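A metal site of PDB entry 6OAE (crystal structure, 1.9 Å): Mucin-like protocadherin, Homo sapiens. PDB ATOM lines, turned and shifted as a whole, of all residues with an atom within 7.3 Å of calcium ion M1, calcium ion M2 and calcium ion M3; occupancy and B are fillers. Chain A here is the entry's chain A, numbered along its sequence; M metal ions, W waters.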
ATOM      1  N   GLU A  17      25.666  35.188 -14.340  1.00  0.00           N
ATOM      2  CA  GLU A  17      27.081  35.312 -14.763  1.00  0.00           C
ATOM      3  C   GLU A  17      27.107  35.788 -16.202  1.00  0.00           C
ATOM      4  O   GLU A  17      26.118  35.547 -16.938  1.00  0.00           O
ATOM      5  CB  GLU A  17      27.841  34.006 -14.574  1.00  0.00           C
ATOM      6  CG  GLU A  17      27.268  32.835 -15.357  1.00  0.00           C
ATOM      7  CD  GLU A  17      28.234  31.674 -15.446  1.00  0.00           C
ATOM      8  OE1 GLU A  17      27.754  30.546 -15.621  1.00  0.00           O
ATOM      9  OE2 GLU A  17      29.444  31.911 -15.346  1.00  0.00           O
ATOM     10  N   ASN A  18      28.188  36.474 -16.582  1.00  0.00           N
ATOM     11  CA  ASN A  18      28.426  37.039 -17.940  1.00  0.00           C
ATOM     12  C   ASN A  18      27.522  38.254 -18.190  1.00  0.00           C
ATOM     13  O   ASN A  18      27.544  38.733 -19.307  1.00  0.00           O
ATOM     14  CB  ASN A  18      28.303  35.963 -19.028  1.00  0.00           C
ATOM     15  CG  ASN A  18      29.175  34.765 -18.707  1.00  0.00           C
ATOM     16  OD1 ASN A  18      30.254  34.928 -18.148  1.00  0.00           O
ATOM     17  ND2 ASN A  18      28.715  33.578 -19.054  1.00  0.00           N
ATOM     18  N   PRO A  60      30.596  38.982 -13.634  1.00  0.00           N
ATOM     19  CA  PRO A  60      30.810  37.794 -12.818  1.00  0.00           C
ATOM     20  C   PRO A  60      30.930  36.501 -13.629  1.00  0.00           C
ATOM     21  O   PRO A  60      30.415  36.438 -14.758  1.00  0.00           O
ATOM     22  CB  PRO A  60      29.538  37.680 -11.958  1.00  0.00           C
ATOM     23  CG  PRO A  60      28.888  39.022 -12.051  1.00  0.00           C
ATOM     24  CD  PRO A  60      29.278  39.579 -13.393  1.00  0.00           C
ATOM     25  N   ASP A  61      31.611  35.522 -13.043  1.00  0.00           N
ATOM     26  CA  ASP A  61      31.810  34.170 -13.610  1.00  0.00           C
ATOM     27  C   ASP A  61      31.542  33.168 -12.502  1.00  0.00           C
ATOM     28  O   ASP A  61      32.370  33.051 -11.596  1.00  0.00           O
ATOM     29  CB  ASP A  61      33.207  34.019 -14.197  1.00  0.00           C
ATOM     30  CG  ASP A  61      33.550  32.603 -14.655  1.00  0.00           C
ATOM     31  OD1 ASP A  61      32.646  31.770 -14.699  1.00  0.00           O
ATOM     32  OD2 ASP A  61      34.721  32.358 -14.928  1.00  0.00           O
ATOM     33  N   TYR A  62      30.413  32.472 -12.595  1.00  0.00           N
ATOM     34  CA  TYR A  62      29.954  31.467 -11.605  1.00  0.00           C
ATOM     35  C   TYR A  62      31.031  30.402 -11.337  1.00  0.00           C
ATOM     36  O   TYR A  62      31.125  29.925 -10.174  1.00  0.00           O
ATOM     37  CB  TYR A  62      28.661  30.828 -12.064  1.00  0.00           C
ATOM     38  CG  TYR A  62      28.084  29.881 -11.064  1.00  0.00           C
ATOM     39  CD1 TYR A  62      27.223  30.324 -10.076  1.00  0.00           C
ATOM     40  CD2 TYR A  62      28.415  28.530 -11.080  1.00  0.00           C
ATOM     41  CE1 TYR A  62      26.684  29.457  -9.126  1.00  0.00           C
ATOM     42  CE2 TYR A  62      27.888  27.651 -10.144  1.00  0.00           C
ATOM     43  CZ  TYR A  62      27.028  28.123  -9.161  1.00  0.00           C
ATOM     44  OH  TYR A  62      26.512  27.248  -8.246  1.00  0.00           O
ATOM     45  N   GLU A  63      31.835  30.042 -12.348  1.00  0.00           N
ATOM     46  CA  GLU A  63      32.912  29.015 -12.227  1.00  0.00           C
ATOM     47  C   GLU A  63      34.136  29.579 -11.463  1.00  0.00           C
ATOM     48  O   GLU A  63      34.913  28.783 -10.953  1.00  0.00           O
ATOM     49  CB  GLU A  63      33.289  28.495 -13.615  1.00  0.00           C
ATOM     50  CG  GLU A  63      32.290  27.496 -14.201  1.00  0.00           C
ATOM     51  CD  GLU A  63      30.938  28.049 -14.649  1.00  0.00           C
ATOM     52  OE1 GLU A  63      30.921  28.997 -15.467  1.00  0.00           O
ATOM     53  OE2 GLU A  63      29.901  27.524 -14.219  1.00  0.00           O
ATOM     54  N   GLU A  64      34.306  30.901 -11.394  1.00  0.00           N
ATOM     55  CA  GLU A  64      35.423  31.543 -10.648  1.00  0.00           C
ATOM     56  C   GLU A  64      34.956  31.875  -9.227  1.00  0.00           C
ATOM     57  O   GLU A  64      35.689  31.530  -8.275  1.00  0.00           O
ATOM     58  CB  GLU A  64      35.906  32.754 -11.460  1.00  0.00           C
ATOM     59  CG  GLU A  64      37.048  33.540 -10.820  1.00  0.00           C
ATOM     60  CD  GLU A  64      36.644  34.796 -10.068  1.00  0.00           C
ATOM     61  OE1 GLU A  64      35.656  35.463 -10.472  1.00  0.00           O
ATOM     62  OE2 GLU A  64      37.329  35.127  -9.069  1.00  0.00           O
ATOM     63  N   LEU A  91      24.364  33.742 -10.534  1.00  0.00           N
ATOM     64  CA  LEU A  91      23.546  32.607 -11.023  1.00  0.00           C
ATOM     65  C   LEU A  91      24.293  31.923 -12.163  1.00  0.00           C
ATOM     66  O   LEU A  91      24.801  32.624 -13.074  1.00  0.00           O
ATOM     67  CB  LEU A  91      22.178  33.089 -11.506  1.00  0.00           C
ATOM     68  CG  LEU A  91      21.338  33.855 -10.478  1.00  0.00           C
ATOM     69  CD1 LEU A  91      19.981  34.210 -11.084  1.00  0.00           C
ATOM     70  CD2 LEU A  91      21.172  33.060  -9.194  1.00  0.00           C
ATOM     71  N   ASP A  92      24.336  30.609 -12.107  1.00  0.00           N
ATOM     72  CA  ASP A  92      25.009  29.790 -13.131  1.00  0.00           C
ATOM     73  C   ASP A  92      24.222  29.867 -14.436  1.00  0.00           C
ATOM     74  O   ASP A  92      22.953  29.842 -14.427  1.00  0.00           O
ATOM     75  CB  ASP A  92      25.190  28.340 -12.670  1.00  0.00           C
ATOM     76  CG  ASP A  92      25.910  27.499 -13.707  1.00  0.00           C
ATOM     77  OD1 ASP A  92      26.895  28.035 -14.334  1.00  0.00           O
ATOM     78  OD2 ASP A  92      25.470  26.343 -13.936  1.00  0.00           O
ATOM     79  N   VAL A  93      24.962  29.979 -15.528  1.00  0.00           N
ATOM     80  CA  VAL A  93      24.483  29.921 -16.930  1.00  0.00           C
ATOM     81  C   VAL A  93      25.186  28.712 -17.572  1.00  0.00           C
ATOM     82  O   VAL A  93      26.341  28.388 -17.166  1.00  0.00           O
ATOM     83  CB  VAL A  93      24.807  31.249 -17.650  1.00  0.00           C
ATOM     84  CG1 VAL A  93      24.694  31.144 -19.171  1.00  0.00           C
ATOM     85  CG2 VAL A  93      23.933  32.385 -17.114  1.00  0.00           C
ATOM     86  N   ASN A  94      24.518  28.055 -18.513  1.00  0.00           N
ATOM     87  CA  ASN A  94      25.136  26.967 -19.311  1.00  0.00           C
ATOM     88  C   ASN A  94      26.064  27.651 -20.331  1.00  0.00           C
ATOM     89  O   ASN A  94      25.625  27.883 -21.477  1.00  0.00           O
ATOM     90  CB  ASN A  94      24.071  26.047 -19.931  1.00  0.00           C
ATOM     91  CG  ASN A  94      24.678  24.926 -20.745  1.00  0.00           C
ATOM     92  OD1 ASN A  94      25.885  24.727 -20.671  1.00  0.00           O
ATOM     93  ND2 ASN A  94      23.871  24.204 -21.504  1.00  0.00           N
ATOM     94  N   ASP A  95      27.286  27.994 -19.918  1.00  0.00           N
ATOM     95  CA  ASP A  95      28.236  28.792 -20.739  1.00  0.00           C
ATOM     96  C   ASP A  95      29.488  27.989 -21.111  1.00  0.00           C
ATOM     97  O   ASP A  95      30.397  28.581 -21.734  1.00  0.00           O
ATOM     98  CB  ASP A  95      28.579  30.125 -20.050  1.00  0.00           C
ATOM     99  CG  ASP A  95      29.285  30.032 -18.706  1.00  0.00           C
ATOM    100  OD1 ASP A  95      29.154  29.003 -18.030  1.00  0.00           O
ATOM    101  OD2 ASP A  95      29.980  31.040 -18.321  1.00  0.00           O
ATOM    102  N   ASN A  96      29.543  26.690 -20.763  1.00  0.00           N
ATOM    103  CA  ASN A  96      30.682  25.783 -21.048  1.00  0.00           C
ATOM    104  C   ASN A  96      30.157  24.573 -21.836  1.00  0.00           C
ATOM    105  O   ASN A  96      29.034  24.109 -21.556  1.00  0.00           O
ATOM    106  CB  ASN A  96      31.387  25.361 -19.758  1.00  0.00           C
ATOM    107  CG  ASN A  96      32.116  26.527 -19.114  1.00  0.00           C
ATOM    108  OD1 ASN A  96      33.245  26.839 -19.492  1.00  0.00           O
ATOM    109  ND2 ASN A  96      31.488  27.178 -18.166  1.00  0.00           N
ATOM    110  N   ALA A  97      30.949  24.118 -22.806  1.00  0.00           N
ATOM    111  CA  ALA A  97      30.618  22.931 -23.639  1.00  0.00           C
ATOM    112  C   ALA A  97      31.248  21.702 -22.988  1.00  0.00           C
ATOM    113  O   ALA A  97      32.321  21.793 -22.362  1.00  0.00           O
ATOM    114  CB  ALA A  97      31.095  23.134 -25.054  1.00  0.00           C
ATOM    115  N   PRO A  98      30.609  20.523 -23.068  1.00  0.00           N
ATOM    116  CA  PRO A  98      31.245  19.297 -22.604  1.00  0.00           C
ATOM    117  C   PRO A  98      32.378  18.983 -23.583  1.00  0.00           C
ATOM    118  O   PRO A  98      32.286  19.322 -24.746  1.00  0.00           O
ATOM    119  CB  PRO A  98      30.117  18.245 -22.592  1.00  0.00           C
ATOM    120  CG  PRO A  98      29.128  18.767 -23.630  1.00  0.00           C
ATOM    121  CD  PRO A  98      29.253  20.278 -23.584  1.00  0.00           C
ATOM    122  N   ASP A 129      32.385  18.857 -18.242  1.00  0.00           N
ATOM    123  CA  ASP A 129      31.761  20.165 -18.523  1.00  0.00           C
ATOM    124  C   ASP A 129      32.044  21.066 -17.323  1.00  0.00           C
ATOM    125  O   ASP A 129      31.671  20.668 -16.187  1.00  0.00           O
ATOM    126  CB  ASP A 129      30.272  19.923 -18.800  1.00  0.00           C
ATOM    127  CG  ASP A 129      29.526  21.137 -19.271  1.00  0.00           C
ATOM    128  OD1 ASP A 129      29.815  22.253 -18.769  1.00  0.00           O
ATOM    129  OD2 ASP A 129      28.648  20.958 -20.134  1.00  0.00           O
ATOM    130  N   ARG A 130      32.677  22.225 -17.548  1.00  0.00           N
ATOM    131  CA  ARG A 130      33.059  23.170 -16.456  1.00  0.00           C
ATOM    132  C   ARG A 130      31.809  23.773 -15.798  1.00  0.00           C
ATOM    133  O   ARG A 130      31.964  24.388 -14.738  1.00  0.00           O
ATOM    134  CB  ARG A 130      34.055  24.220 -16.978  1.00  0.00           C
ATOM    135  CG  ARG A 130      35.416  23.641 -17.356  1.00  0.00           C
ATOM    136  CD  ARG A 130      36.412  24.702 -17.793  1.00  0.00           C
ATOM    137  NE  ARG A 130      37.722  24.132 -18.089  1.00  0.00           N
ATOM    138  CZ  ARG A 130      38.580  23.692 -17.178  1.00  0.00           C
ATOM    139  NH1 ARG A 130      39.744  23.173 -17.555  1.00  0.00           N
ATOM    140  NH2 ARG A 130      38.297  23.775 -15.883  1.00  0.00           N
ATOM    141  N   ASP A 131      30.615  23.620 -16.359  1.00  0.00           N
ATOM    142  CA  ASP A 131      29.345  23.830 -15.622  1.00  0.00           C
ATOM    143  C   ASP A 131      29.182  22.597 -14.729  1.00  0.00           C
ATOM    144  O   ASP A 131      28.610  21.590 -15.194  1.00  0.00           O
ATOM    145  CB  ASP A 131      28.164  24.032 -16.559  1.00  0.00           C
ATOM    146  CG  ASP A 131      28.340  25.207 -17.489  1.00  0.00           C
ATOM    147  OD1 ASP A 131      28.714  26.285 -16.977  1.00  0.00           O
ATOM    148  OD2 ASP A 131      28.123  25.052 -18.705  1.00  0.00           O
ATOM    149  N   LYS A 132      29.676  22.662 -13.502  1.00  0.00           N
ATOM    150  CA  LYS A 132      29.777  21.492 -12.593  1.00  0.00           C
ATOM    151  C   LYS A 132      28.398  20.837 -12.379  1.00  0.00           C
ATOM    152  O   LYS A 132      28.365  19.644 -12.118  1.00  0.00           O
ATOM    153  CB  LYS A 132      30.323  21.916 -11.230  1.00  0.00           C
ATOM    154  CG  LYS A 132      31.797  22.295 -11.179  1.00  0.00           C
ATOM    155  CD  LYS A 132      32.378  22.203  -9.763  1.00  0.00           C
ATOM    156  CE  LYS A 132      32.124  23.418  -8.877  1.00  0.00           C
ATOM    157  NZ  LYS A 132      30.702  23.838  -8.785  1.00  0.00           N
ATOM    158  N   ASP A 134      25.888  20.580 -14.590  1.00  0.00           N
ATOM    159  CA  ASP A 134      25.283  20.051 -15.843  1.00  0.00           C
ATOM    160  C   ASP A 134      25.320  18.516 -15.806  1.00  0.00           C
ATOM    161  O   ASP A 134      26.410  17.970 -15.565  1.00  0.00           O
ATOM    162  CB  ASP A 134      25.988  20.591 -17.091  1.00  0.00           C
ATOM    163  CG  ASP A 134      25.587  22.000 -17.486  1.00  0.00           C
ATOM    164  OD1 ASP A 134      24.764  22.612 -16.756  1.00  0.00           O
ATOM    165  OD2 ASP A 134      26.069  22.466 -18.541  1.00  0.00           O
ATOM    166  N   LEU A 136      25.240  15.250 -18.022  1.00  0.00           N
ATOM    167  CA  LEU A 136      25.619  15.002 -19.432  1.00  0.00           C
ATOM    168  C   LEU A 136      24.843  13.791 -19.955  1.00  0.00           C
ATOM    169  O   LEU A 136      24.653  12.826 -19.214  1.00  0.00           O
ATOM    170  CB  LEU A 136      27.139  14.820 -19.516  1.00  0.00           C
ATOM    171  CG  LEU A 136      27.944  16.031 -19.039  1.00  0.00           C
ATOM    172  CD1 LEU A 136      29.418  15.853 -19.363  1.00  0.00           C
ATOM    173  CD2 LEU A 136      27.420  17.332 -19.627  1.00  0.00           C
ATOM    174  N   ARG A 182      25.803  15.737 -24.869  1.00  0.00           N
ATOM    175  CA  ARG A 182      25.207  17.098 -24.769  1.00  0.00           C
ATOM    176  C   ARG A 182      25.006  17.380 -23.285  1.00  0.00           C
ATOM    177  O   ARG A 182      24.941  16.406 -22.482  1.00  0.00           O
ATOM    178  CB  ARG A 182      23.931  17.221 -25.607  1.00  0.00           C
ATOM    179  CG  ARG A 182      22.804  16.311 -25.179  1.00  0.00           C
ATOM    180  CD  ARG A 182      21.443  16.568 -25.827  1.00  0.00           C
ATOM    181  NE  ARG A 182      20.457  15.682 -25.197  1.00  0.00           N
ATOM    182  CZ  ARG A 182      20.210  14.404 -25.535  1.00  0.00           C
ATOM    183  NH1 ARG A 182      20.839  13.817 -26.541  1.00  0.00           N
ATOM    184  NH2 ARG A 182      19.304  13.729 -24.869  1.00  0.00           N
ATOM    185  N   ASP A 183      24.900  18.668 -22.923  1.00  0.00           N
ATOM    186  CA  ASP A 183      24.781  19.104 -21.510  1.00  0.00           C
ATOM    187  C   ASP A 183      23.331  19.483 -21.184  1.00  0.00           C
ATOM    188  O   ASP A 183      23.127  20.162 -20.190  1.00  0.00           O
ATOM    189  CB  ASP A 183      25.760  20.234 -21.223  1.00  0.00           C
ATOM    190  CG  ASP A 183      25.640  21.455 -22.128  1.00  0.00           C
ATOM    191  OD1 ASP A 183      24.691  21.510 -22.968  1.00  0.00           O
ATOM    192  OD2 ASP A 183      26.526  22.320 -21.991  1.00  0.00           O
ATOM    193  N   THR A 184      22.357  19.061 -21.995  1.00  0.00           N
ATOM    194  CA  THR A 184      20.905  19.296 -21.774  1.00  0.00           C
ATOM    195  C   THR A 184      20.142  18.010 -22.057  1.00  0.00           C
ATOM    196  O   THR A 184      20.526  17.225 -22.927  1.00  0.00           O
ATOM    197  CB  THR A 184      20.386  20.441 -22.648  1.00  0.00           C
ATOM    198  OG1 THR A 184      20.534  20.091 -24.036  1.00  0.00           O
ATOM    199  CG2 THR A 184      21.090  21.746 -22.331  1.00  0.00           C
ATOM    200  N   SER A 192      22.487  24.816 -25.562  1.00  0.00           N
ATOM    201  CA  SER A 192      22.876  23.379 -25.503  1.00  0.00           C
ATOM    202  C   SER A 192      24.203  23.196 -26.252  1.00  0.00           C
ATOM    203  O   SER A 192      24.325  23.740 -27.339  1.00  0.00           O
ATOM    204  CB  SER A 192      21.807  22.489 -26.064  1.00  0.00           C
ATOM    205  OG  SER A 192      22.193  21.129 -25.956  1.00  0.00           O
ATOM    206  N   HIS A 193      25.134  22.449 -25.692  1.00  0.00           N
ATOM    207  CA  HIS A 193      26.458  22.231 -26.314  1.00  0.00           C
ATOM    208  C   HIS A 193      26.651  20.745 -26.527  1.00  0.00           C
ATOM    209  O   HIS A 193      26.282  19.990 -25.618  1.00  0.00           O
ATOM    210  CB  HIS A 193      27.556  22.796 -25.438  1.00  0.00           C
ATOM    211  CG  HIS A 193      27.314  24.204 -25.018  1.00  0.00           C
ATOM    212  ND1 HIS A 193      26.870  24.505 -23.763  1.00  0.00           N
ATOM    213  CD2 HIS A 193      27.438  25.378 -25.691  1.00  0.00           C
ATOM    214  CE1 HIS A 193      26.739  25.819 -23.650  1.00  0.00           C
ATOM    215  NE2 HIS A 193      27.068  26.376 -24.837  1.00  0.00           N
HETATM  216 CA    CA M   1      28.377  28.318 -15.985  1.00  0.00          CA
HETATM  217 CA    CA M   2      31.279  31.034 -16.527  1.00  0.00          CA
HETATM  218 CA    CA M   3      27.557  23.161 -20.088  1.00  0.00          CA
HETATM  219  O   HOH W   1      32.090  33.121 -17.416  1.00  0.00           O
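The backbone NH of Glu 17 lies within hydrogen-bond range of the backbone carbonyl oxygen of Leu 91.
ND1 of His 193 lies close to O of Asn 96, at 3.1 Å.
OD1 of Asp 183 lies within hydrogen-bond range of N of His 193, at 2.9 Å.
OD2 of Asp 95 lies close to ND2 of Asn 18 (2.9 Å).
OD1 of Asn 94 sits close to ND1 of His 193 (3.3 Å).
ND2 of Asn 96 lies close to OD1 of Asp 95.
The side-chain carboxylate (OE2) of Glu 17 sits close to the backbone NH (N) of Tyr 62 (3.0 Å).
ND2 of Asn 96 lies close to OE1 of Glu 63 (3.3 Å).
Of the 26 residues printed, 7 come within 4 Å of calcium ion M1.
Of the 26 residues printed, 4 come within 4 Å of calcium ion M2.
Along chain A the residues within 4 Å of calcium ion M2 span positions 17 to 95.
Merely in contact with calcium ion M3: His 193 (3.97 Å).
The nearest printed residue that does not touch calcium ion M3 is Ala 97 (4.5 Å).
OD1 of Asp 92 binds calcium ion M1, at 2.2 Å.
Calcium ion M1 is bound by OD1 of Asp 131, 2.3 Å away.
The side-chain carboxylate (OD1) of Asp 95 binds calcium ion M1 (2.3 Å).
Calcium ion M1 is bound by OE1 of Glu 17 (2.3 Å).
Calcium ion M1 is bound by O of Val 93.
OE2 of Glu 63 is bound to calcium ion M1 (2.5 Å).
The side-chain carboxylate (OE1) of Glu 63 is bound to calcium ion M1, at 2.7 Å.
Calcium ion M2 is bound by OD2 of Asp 95 (2.2 Å), OE1 of Glu 63 (2.3 Å), OE2 of Glu 17 (2.4 Å), OD1 of Asp 61 (2.4 Å) and water W1 (2.4 Å).
Calcium ion M2 has five donor atoms within binding distance.
Calcium ion M3 is bound by OD2 of Asp 134 (2.3 Å), O of Asn 96 (2.3 Å), OD2 of Asp 183 (2.3 Å), OD1 of Asn 94 (2.4 Å), OD2 of Asp 131 (2.4 Å), OD2 of Asp 129 (2.5 Å) and OD1 of Asp 129 (2.8 Å).
Calcium ion M3 has seven donor atoms within binding distance.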
